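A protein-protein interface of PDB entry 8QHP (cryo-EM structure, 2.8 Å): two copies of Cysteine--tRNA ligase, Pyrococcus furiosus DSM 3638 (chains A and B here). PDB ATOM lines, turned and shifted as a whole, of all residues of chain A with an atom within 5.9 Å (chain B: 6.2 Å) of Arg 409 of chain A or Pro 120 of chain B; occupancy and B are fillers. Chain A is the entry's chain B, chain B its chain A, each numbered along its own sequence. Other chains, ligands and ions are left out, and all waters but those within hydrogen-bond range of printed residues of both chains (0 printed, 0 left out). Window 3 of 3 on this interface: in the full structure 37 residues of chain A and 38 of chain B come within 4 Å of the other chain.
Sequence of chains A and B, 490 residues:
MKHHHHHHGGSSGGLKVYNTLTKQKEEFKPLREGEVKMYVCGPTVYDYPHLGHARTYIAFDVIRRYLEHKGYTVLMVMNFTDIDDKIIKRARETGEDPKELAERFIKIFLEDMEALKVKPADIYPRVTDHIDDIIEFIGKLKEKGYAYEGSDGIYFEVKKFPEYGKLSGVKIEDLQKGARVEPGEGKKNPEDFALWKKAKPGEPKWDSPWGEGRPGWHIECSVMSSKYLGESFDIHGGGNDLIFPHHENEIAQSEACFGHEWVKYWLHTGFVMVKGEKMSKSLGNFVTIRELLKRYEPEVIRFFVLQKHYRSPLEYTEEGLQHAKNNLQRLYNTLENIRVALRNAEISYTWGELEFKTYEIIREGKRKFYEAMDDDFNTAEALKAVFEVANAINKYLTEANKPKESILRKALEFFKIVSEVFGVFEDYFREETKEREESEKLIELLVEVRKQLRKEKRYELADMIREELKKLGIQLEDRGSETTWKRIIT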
ATOM      1  N   LEU A 342       1.815   3.070  -8.705  1.00  0.00           N
ATOM      2  CA  LEU A 342       1.288   3.293 -10.048  1.00  0.00           C
ATOM      3  C   LEU A 342       1.183   4.769 -10.404  1.00  0.00           C
ATOM      4  O   LEU A 342       1.110   5.099 -11.592  1.00  0.00           O
ATOM      5  CB  LEU A 342      -0.083   2.635 -10.195  1.00  0.00           C
ATOM      6  CG  LEU A 342      -0.081   1.215 -10.752  1.00  0.00           C
ATOM      7  CD1 LEU A 342      -1.498   0.698 -10.871  1.00  0.00           C
ATOM      8  CD2 LEU A 342       0.615   1.181 -12.099  1.00  0.00           C
ATOM      9  N   ILE A 347       6.418   3.919 -18.284  1.00  0.00           N
ATOM     10  CA  ILE A 347       6.338   2.849 -19.270  1.00  0.00           C
ATOM     11  C   ILE A 347       7.694   2.165 -19.406  1.00  0.00           C
ATOM     12  O   ILE A 347       8.738   2.693 -19.008  1.00  0.00           O
ATOM     13  CB  ILE A 347       5.849   3.382 -20.624  1.00  0.00           C
ATOM     14  CG1 ILE A 347       6.846   4.394 -21.185  1.00  0.00           C
ATOM     15  CG2 ILE A 347       4.474   4.009 -20.484  1.00  0.00           C
ATOM     16  CD1 ILE A 347       6.457   4.928 -22.536  1.00  0.00           C
ATOM     17  N   LYS A 404       8.119  -0.229 -13.099  1.00  0.00           N
ATOM     18  CA  LYS A 404       7.527  -0.237 -14.426  1.00  0.00           C
ATOM     19  C   LYS A 404       6.015  -0.359 -14.322  1.00  0.00           C
ATOM     20  O   LYS A 404       5.494  -1.057 -13.449  1.00  0.00           O
ATOM     21  CB  LYS A 404       8.087  -1.387 -15.262  1.00  0.00           C
ATOM     22  CG  LYS A 404       9.594  -1.354 -15.440  1.00  0.00           C
ATOM     23  CD  LYS A 404      10.052  -0.058 -16.077  1.00  0.00           C
ATOM     24  CE  LYS A 404      11.560  -0.034 -16.235  1.00  0.00           C
ATOM     25  NZ  LYS A 404      12.032   1.254 -16.805  1.00  0.00           N
ATOM     26  N   GLU A 405       5.311   0.327 -15.224  1.00  0.00           N
ATOM     27  CA  GLU A 405       3.855   0.301 -15.188  1.00  0.00           C
ATOM     28  C   GLU A 405       3.303  -1.052 -15.617  1.00  0.00           C
ATOM     29  O   GLU A 405       2.253  -1.470 -15.123  1.00  0.00           O
ATOM     30  CB  GLU A 405       3.292   1.414 -16.071  1.00  0.00           C
ATOM     31  CG  GLU A 405       1.790   1.606 -15.948  1.00  0.00           C
ATOM     32  CD  GLU A 405       1.006   0.759 -16.930  1.00  0.00           C
ATOM     33  OE1 GLU A 405       1.619   0.209 -17.868  1.00  0.00           O
ATOM     34  OE2 GLU A 405      -0.226   0.643 -16.760  1.00  0.00           O
ATOM     35  N   SER A 406       3.987  -1.743 -16.532  1.00  0.00           N
ATOM     36  CA  SER A 406       3.475  -3.018 -17.029  1.00  0.00           C
ATOM     37  C   SER A 406       3.474  -4.088 -15.942  1.00  0.00           C
ATOM     38  O   SER A 406       2.517  -4.863 -15.832  1.00  0.00           O
ATOM     39  CB  SER A 406       4.294  -3.475 -18.233  1.00  0.00           C
ATOM     40  OG  SER A 406       5.682  -3.439 -17.952  1.00  0.00           O
ATOM     41  N   ILE A 407       4.533  -4.150 -15.134  1.00  0.00           N
ATOM     42  CA  ILE A 407       4.602  -5.150 -14.071  1.00  0.00           C
ATOM     43  C   ILE A 407       3.496  -4.919 -13.048  1.00  0.00           C
ATOM     44  O   ILE A 407       2.806  -5.855 -12.626  1.00  0.00           O
ATOM     45  CB  ILE A 407       5.993  -5.130 -13.413  1.00  0.00           C
ATOM     46  CG1 ILE A 407       7.060  -5.588 -14.408  1.00  0.00           C
ATOM     47  CG2 ILE A 407       6.012  -6.003 -12.174  1.00  0.00           C
ATOM     48  CD1 ILE A 407       6.912  -7.025 -14.839  1.00  0.00           C
ATOM     49  N   LEU A 408       3.306  -3.662 -12.641  1.00  0.00           N
ATOM     50  CA  LEU A 408       2.246  -3.347 -11.693  1.00  0.00           C
ATOM     51  C   LEU A 408       0.874  -3.620 -12.292  1.00  0.00           C
ATOM     52  O   LEU A 408      -0.038  -4.067 -11.588  1.00  0.00           O
ATOM     53  CB  LEU A 408       2.361  -1.893 -11.243  1.00  0.00           C
ATOM     54  CG  LEU A 408       3.699  -1.510 -10.614  1.00  0.00           C
ATOM     55  CD1 LEU A 408       3.680  -0.064 -10.161  1.00  0.00           C
ATOM     56  CD2 LEU A 408       4.019  -2.434  -9.455  1.00  0.00           C
ATOM     57  N   ARG A 409       0.707  -3.361 -13.590  1.00  0.00           N
ATOM     58  CA  ARG A 409      -0.570  -3.645 -14.236  1.00  0.00           C
ATOM     59  C   ARG A 409      -0.858  -5.140 -14.250  1.00  0.00           C
ATOM     60  O   ARG A 409      -1.996  -5.559 -14.014  1.00  0.00           O
ATOM     61  CB  ARG A 409      -0.584  -3.083 -15.656  1.00  0.00           C
ATOM     62  CG  ARG A 409      -1.943  -3.168 -16.329  1.00  0.00           C
ATOM     63  CD  ARG A 409      -1.900  -2.708 -17.778  1.00  0.00           C
ATOM     64  NE  ARG A 409      -1.149  -3.625 -18.628  1.00  0.00           N
ATOM     65  CZ  ARG A 409       0.040  -3.359 -19.148  1.00  0.00           C
ATOM     66  NH1 ARG A 409       0.640  -2.199 -18.943  1.00  0.00           N
ATOM     67  NH2 ARG A 409       0.638  -4.278 -19.900  1.00  0.00           N
ATOM     68  N   LYS A 410       0.156  -5.961 -14.527  1.00  0.00           N
ATOM     69  CA  LYS A 410      -0.043  -7.407 -14.497  1.00  0.00           C
ATOM     70  C   LYS A 410      -0.361  -7.894 -13.089  1.00  0.00           C
ATOM     71  O   LYS A 410      -1.223  -8.767 -12.904  1.00  0.00           O
ATOM     72  CB  LYS A 410       1.187  -8.122 -15.049  1.00  0.00           C
ATOM     73  CG  LYS A 410       1.393  -7.915 -16.537  1.00  0.00           C
ATOM     74  CD  LYS A 410       2.498  -8.807 -17.066  1.00  0.00           C
ATOM     75  CE  LYS A 410       2.598  -8.708 -18.575  1.00  0.00           C
ATOM     76  NZ  LYS A 410       1.305  -9.044 -19.229  1.00  0.00           N
ATOM     77  N   ALA A 411       0.321  -7.342 -12.082  1.00  0.00           N
ATOM     78  CA  ALA A 411       0.012  -7.711 -10.704  1.00  0.00           C
ATOM     79  C   ALA A 411      -1.420  -7.334 -10.344  1.00  0.00           C
ATOM     80  O   ALA A 411      -2.135  -8.116  -9.706  1.00  0.00           O
ATOM     81  CB  ALA A 411       1.001  -7.048  -9.747  1.00  0.00           C
ATOM     82  N   LEU A 412      -1.860  -6.145 -10.759  1.00  0.00           N
ATOM     83  CA  LEU A 412      -3.232  -5.732 -10.492  1.00  0.00           C
ATOM     84  C   LEU A 412      -4.238  -6.594 -11.238  1.00  0.00           C
ATOM     85  O   LEU A 412      -5.323  -6.853 -10.717  1.00  0.00           O
ATOM     86  CB  LEU A 412      -3.434  -4.263 -10.853  1.00  0.00           C
ATOM     87  CG  LEU A 412      -3.114  -3.247  -9.757  1.00  0.00           C
ATOM     88  CD1 LEU A 412      -3.811  -1.933 -10.046  1.00  0.00           C
ATOM     89  CD2 LEU A 412      -3.519  -3.780  -8.397  1.00  0.00           C
ATOM     90  N   GLU A 413      -3.914  -7.035 -12.453  1.00  0.00           N
ATOM     91  CA  GLU A 413      -4.812  -7.939 -13.166  1.00  0.00           C
ATOM     92  C   GLU A 413      -4.938  -9.275 -12.444  1.00  0.00           C
ATOM     93  O   GLU A 413      -6.042  -9.824 -12.321  1.00  0.00           O
ATOM     94  CB  GLU A 413      -4.326  -8.144 -14.599  1.00  0.00           C
ATOM     95  CG  GLU A 413      -4.487  -6.923 -15.487  1.00  0.00           C
ATOM     96  CD  GLU A 413      -3.848  -7.110 -16.847  1.00  0.00           C
ATOM     97  OE1 GLU A 413      -3.255  -8.183 -17.081  1.00  0.00           O
ATOM     98  OE2 GLU A 413      -3.936  -6.185 -17.681  1.00  0.00           O
ATOM     99  N   PHE A 414      -3.819  -9.810 -11.953  1.00  0.00           N
ATOM    100  CA  PHE A 414      -3.884 -11.053 -11.187  1.00  0.00           C
ATOM    101  C   PHE A 414      -4.710 -10.874  -9.919  1.00  0.00           C
ATOM    102  O   PHE A 414      -5.550 -11.722  -9.587  1.00  0.00           O
ATOM    103  CB  PHE A 414      -2.478 -11.542 -10.849  1.00  0.00           C
ATOM    104  CG  PHE A 414      -2.455 -12.675  -9.868  1.00  0.00           C
ATOM    105  CD1 PHE A 414      -2.820 -13.950 -10.256  1.00  0.00           C
ATOM    106  CD2 PHE A 414      -2.069 -12.466  -8.557  1.00  0.00           C
ATOM    107  CE1 PHE A 414      -2.804 -14.992  -9.353  1.00  0.00           C
ATOM    108  CE2 PHE A 414      -2.049 -13.505  -7.652  1.00  0.00           C
ATOM    109  CZ  PHE A 414      -2.417 -14.769  -8.051  1.00  0.00           C
ATOM    110  N   ASP B  61      -5.355  -5.295 -29.657  1.00  0.00           N
ATOM    111  CA  ASP B  61      -5.713  -5.083 -28.261  1.00  0.00           C
ATOM    112  C   ASP B  61      -6.880  -5.973 -27.862  1.00  0.00           C
ATOM    113  O   ASP B  61      -6.908  -6.508 -26.751  1.00  0.00           O
ATOM    114  CB  ASP B  61      -6.048  -3.613 -28.023  1.00  0.00           C
ATOM    115  CG  ASP B  61      -6.421  -3.327 -26.588  1.00  0.00           C
ATOM    116  OD1 ASP B  61      -5.578  -3.565 -25.700  1.00  0.00           O
ATOM    117  OD2 ASP B  61      -7.553  -2.857 -26.348  1.00  0.00           O
ATOM    118  N   ARG B  64      -5.496  -9.407 -27.441  1.00  0.00           N
ATOM    119  CA  ARG B  64      -4.817  -9.508 -26.155  1.00  0.00           C
ATOM    120  C   ARG B  64      -5.818  -9.617 -25.013  1.00  0.00           C
ATOM    121  O   ARG B  64      -5.646 -10.430 -24.099  1.00  0.00           O
ATOM    122  CB  ARG B  64      -3.897  -8.306 -25.948  1.00  0.00           C
ATOM    123  CG  ARG B  64      -3.070  -8.401 -24.691  1.00  0.00           C
ATOM    124  CD  ARG B  64      -3.321  -7.205 -23.824  1.00  0.00           C
ATOM    125  NE  ARG B  64      -2.481  -6.086 -24.234  1.00  0.00           N
ATOM    126  CZ  ARG B  64      -1.311  -5.794 -23.687  1.00  0.00           C
ATOM    127  NH1 ARG B  64      -0.820  -6.516 -22.701  1.00  0.00           N
ATOM    128  NH2 ARG B  64      -0.621  -4.748 -24.136  1.00  0.00           N
ATOM    129  N   GLU B  68      -6.181 -12.785 -22.458  1.00  0.00           N
ATOM    130  CA  GLU B  68      -6.113 -12.646 -21.008  1.00  0.00           C
ATOM    131  C   GLU B  68      -7.413 -13.077 -20.343  1.00  0.00           C
ATOM    132  O   GLU B  68      -7.397 -13.562 -19.207  1.00  0.00           O
ATOM    133  CB  GLU B  68      -5.782 -11.206 -20.628  1.00  0.00           C
ATOM    134  CG  GLU B  68      -4.406 -10.753 -21.063  1.00  0.00           C
ATOM    135  CD  GLU B  68      -4.172  -9.286 -20.793  1.00  0.00           C
ATOM    136  OE1 GLU B  68      -5.165  -8.561 -20.570  1.00  0.00           O
ATOM    137  OE2 GLU B  68      -3.000  -8.857 -20.799  1.00  0.00           O
ATOM    138  N   VAL B  74      -0.355 -12.681 -20.979  1.00  0.00           N
ATOM    139  CA  VAL B  74       0.071 -12.203 -22.288  1.00  0.00           C
ATOM    140  C   VAL B  74       1.184 -11.184 -22.096  1.00  0.00           C
ATOM    141  O   VAL B  74       0.986 -10.144 -21.457  1.00  0.00           O
ATOM    142  CB  VAL B  74      -1.096 -11.599 -23.081  1.00  0.00           C
ATOM    143  CG1 VAL B  74      -0.601 -11.066 -24.413  1.00  0.00           C
ATOM    144  CG2 VAL B  74      -2.178 -12.639 -23.292  1.00  0.00           C
ATOM    145  N   MET B  76       3.046  -8.728 -24.258  1.00  0.00           N
ATOM    146  CA  MET B  76       2.923  -8.084 -25.558  1.00  0.00           C
ATOM    147  C   MET B  76       4.049  -7.078 -25.741  1.00  0.00           C
ATOM    148  O   MET B  76       4.241  -6.191 -24.904  1.00  0.00           O
ATOM    149  CB  MET B  76       1.563  -7.400 -25.706  1.00  0.00           C
ATOM    150  CG  MET B  76       1.097  -7.266 -27.150  1.00  0.00           C
ATOM    151  SD  MET B  76       1.389  -5.640 -27.869  1.00  0.00           S
ATOM    152  CE  MET B  76      -0.158  -4.823 -27.487  1.00  0.00           C
ATOM    153  N   LEU B 110       1.416   7.440 -28.327  1.00  0.00           N
ATOM    154  CA  LEU B 110       1.021   6.897 -27.033  1.00  0.00           C
ATOM    155  C   LEU B 110      -0.235   7.578 -26.512  1.00  0.00           C
ATOM    156  O   LEU B 110      -1.125   6.914 -25.968  1.00  0.00           O
ATOM    157  CB  LEU B 110       2.168   7.031 -26.033  1.00  0.00           C
ATOM    158  CG  LEU B 110       3.332   6.069 -26.265  1.00  0.00           C
ATOM    159  CD1 LEU B 110       4.425   6.291 -25.238  1.00  0.00           C
ATOM    160  CD2 LEU B 110       2.846   4.630 -26.232  1.00  0.00           C
ATOM    161  N   VAL B 118      -6.719   1.590 -25.744  1.00  0.00           N
ATOM    162  CA  VAL B 118      -5.865   0.457 -26.074  1.00  0.00           C
ATOM    163  C   VAL B 118      -4.890   0.232 -24.928  1.00  0.00           C
ATOM    164  O   VAL B 118      -4.206   1.162 -24.487  1.00  0.00           O
ATOM    165  CB  VAL B 118      -5.124   0.701 -27.397  1.00  0.00           C
ATOM    166  CG1 VAL B 118      -4.180  -0.447 -27.693  1.00  0.00           C
ATOM    167  CG2 VAL B 118      -6.116   0.881 -28.531  1.00  0.00           C
ATOM    168  N   LYS B 119      -4.836  -0.999 -24.434  1.00  0.00           N
ATOM    169  CA  LYS B 119      -3.929  -1.318 -23.340  1.00  0.00           C
ATOM    170  C   LYS B 119      -2.488  -1.163 -23.806  1.00  0.00           C
ATOM    171  O   LYS B 119      -2.118  -1.710 -24.852  1.00  0.00           O
ATOM    172  CB  LYS B 119      -4.170  -2.738 -22.839  1.00  0.00           C
ATOM    173  CG  LYS B 119      -5.543  -2.959 -22.240  1.00  0.00           C
ATOM    174  CD  LYS B 119      -5.709  -4.393 -21.775  1.00  0.00           C
ATOM    175  CE  LYS B 119      -4.652  -4.765 -20.752  1.00  0.00           C
ATOM    176  NZ  LYS B 119      -4.806  -6.172 -20.294  1.00  0.00           N
ATOM    177  N   PRO B 120      -1.650  -0.434 -23.074  1.00  0.00           N
ATOM    178  CA  PRO B 120      -0.266  -0.242 -23.512  1.00  0.00           C
ATOM    179  C   PRO B 120       0.506  -1.549 -23.513  1.00  0.00           C
ATOM    180  O   PRO B 120       0.265  -2.443 -22.700  1.00  0.00           O
ATOM    181  CB  PRO B 120       0.299   0.738 -22.479  1.00  0.00           C
ATOM    182  CG  PRO B 120      -0.544   0.531 -21.270  1.00  0.00           C
ATOM    183  CD  PRO B 120      -1.918   0.218 -21.781  1.00  0.00           C
ATOM    184  N   ALA B 121       1.444  -1.652 -24.449  1.00  0.00           N
ATOM    185  CA  ALA B 121       2.274  -2.840 -24.535  1.00  0.00           C
ATOM    186  C   ALA B 121       3.187  -2.936 -23.319  1.00  0.00           C
ATOM    187  O   ALA B 121       3.539  -1.936 -22.689  1.00  0.00           O
ATOM    188  CB  ALA B 121       3.102  -2.830 -25.819  1.00  0.00           C
ATOM    189  N   ASP B 122       3.562  -4.171 -22.985  1.00  0.00           N
ATOM    190  CA  ASP B 122       4.406  -4.390 -21.816  1.00  0.00           C
ATOM    191  C   ASP B 122       5.797  -3.807 -22.017  1.00  0.00           C
ATOM    192  O   ASP B 122       6.359  -3.200 -21.099  1.00  0.00           O
ATOM    193  CB  ASP B 122       4.484  -5.882 -21.507  1.00  0.00           C
ATOM    194  CG  ASP B 122       3.134  -6.475 -21.176  1.00  0.00           C
ATOM    195  OD1 ASP B 122       2.385  -5.853 -20.396  1.00  0.00           O
ATOM    196  OD2 ASP B 122       2.816  -7.560 -21.703  1.00  0.00           O
ATOM    197  N   TYR B 124       8.296  -1.527 -24.883  1.00  0.00           N
ATOM    198  CA  TYR B 124       8.362  -0.681 -26.074  1.00  0.00           C
ATOM    199  C   TYR B 124       9.827  -0.495 -26.447  1.00  0.00           C
ATOM    200  O   TYR B 124      10.411   0.569 -26.192  1.00  0.00           O
ATOM    201  CB  TYR B 124       7.696   0.673 -25.845  1.00  0.00           C
ATOM    202  CG  TYR B 124       6.187   0.644 -25.825  1.00  0.00           C
ATOM    203  CD1 TYR B 124       5.462   0.578 -27.004  1.00  0.00           C
ATOM    204  CD2 TYR B 124       5.489   0.709 -24.628  1.00  0.00           C
ATOM    205  CE1 TYR B 124       4.083   0.561 -26.993  1.00  0.00           C
ATOM    206  CE2 TYR B 124       4.111   0.692 -24.606  1.00  0.00           C
ATOM    207  CZ  TYR B 124       3.413   0.619 -25.791  1.00  0.00           C
ATOM    208  OH  TYR B 124       2.038   0.603 -25.773  1.00  0.00           O
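N of Lys 119 of chain B is in hydrogen-bond range of OD1 of Asp 61 of chain B, at 3.0 Å. NH1 of Arg 64 of chain B lies within salt-bridge range of OD2 of Asp 122 of chain B (3.9 Å). OE1 of Glu 68 of chain B lies within salt-bridge range of NZ of Lys 119 of chain B (2.4 Å). The backbone NH of Met 76 of chain B sits at hydrogen-bond distance from the side-chain carboxylate of Asp 122 of chain B, 2.8 Å away. The side-chain carboxylate (OE1) of Glu 405 of chain A lies within salt-bridge range of the guanidinium group (NH1) of Arg 409 of chain A, at 2.8 Å. The guanidinium group (NE) of Arg 409 of chain A is in salt-bridge range of the side-chain carboxylate (OE2) of Glu 413 of chain A (3.9 Å).
Of the printed residues of chain B, Arg 409 of chain A touches Arg 64, Pro 120 and Asp 122. Printed residues of chain B within 4 Å of Glu 413 of chain A: Glu 68 (3.8 Å) and Lys 119 (2.8 Å). Printed residues of chain A within 4 Å of Glu 68 of chain B: Glu 413 (3.8 Å). Of the printed residues of chain A, Leu 110 of chain B touches Ile 347. Pro 120 of chain B touches just one residue of chain A: Arg 409 (3.4 Å). The nearest residue of chain B that does not touch Arg 409 of chain A is Lys 119 of chain B (4.3 Å). The nearest residue of chain A that does not touch Pro 120 of chain B is Glu 405 of chain A (4.04 Å).
Among the printed residues, merely in contact across the chains: Ile 347 of chain A with Leu 110 of chain B (3.6 Å), Glu 413 of chain A with Glu 68 of chain B (3.8 Å) and Arg 409 of chain A with Arg 64 of chain B (3.9 Å).
No position is printed for both chains. Of the 9 pairs that touch across the chains among the printed residues, none has its exchanged pair printed and touching as well.
NZ of Lys 410 of chain A sits at hydrogen-bond distance from O of Val 74 of chain B. NZ of Lys 119 of chain B is in salt-bridge range of OE2 of Glu 413 of chain A (2.8 Å). The guanidinium group (NH2) of Arg 409 of chain A is in hydrogen-bond range of the backbone carbonyl oxygen (O) of Pro 120 of chain B, at 3.4 Å. O of Asp 122 of chain B is in hydrogen-bond range of OG of Ser 406 of chain A. The guanidinium group of Arg 409 of chain A lies within salt-bridge range of the side-chain carboxylate of Asp 122 of chain B (2.4 Å). The side-chain carboxylate of Asp 122 of chain B lies within salt-bridge range of the side-chain amino group of Lys 410 of chain A, at 3.3 Å.
Of the 12 printed residues of chain B, 7 touch a printed residue of chain A. Among the printed residues, 9 pairs touch across the chains. Among the printed residues, Asp or Glu carboxylates within 4 Å of a Lys or Arg side-chain nitrogen of the other chain: Arg 409 of chain A with Asp 122 of chain B (2.4 Å), Lys 410 of chain A with Asp 122 of chain B (3.3 Å) and Glu 413 of chain A with Lys 119 of chain B (2.8 Å).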
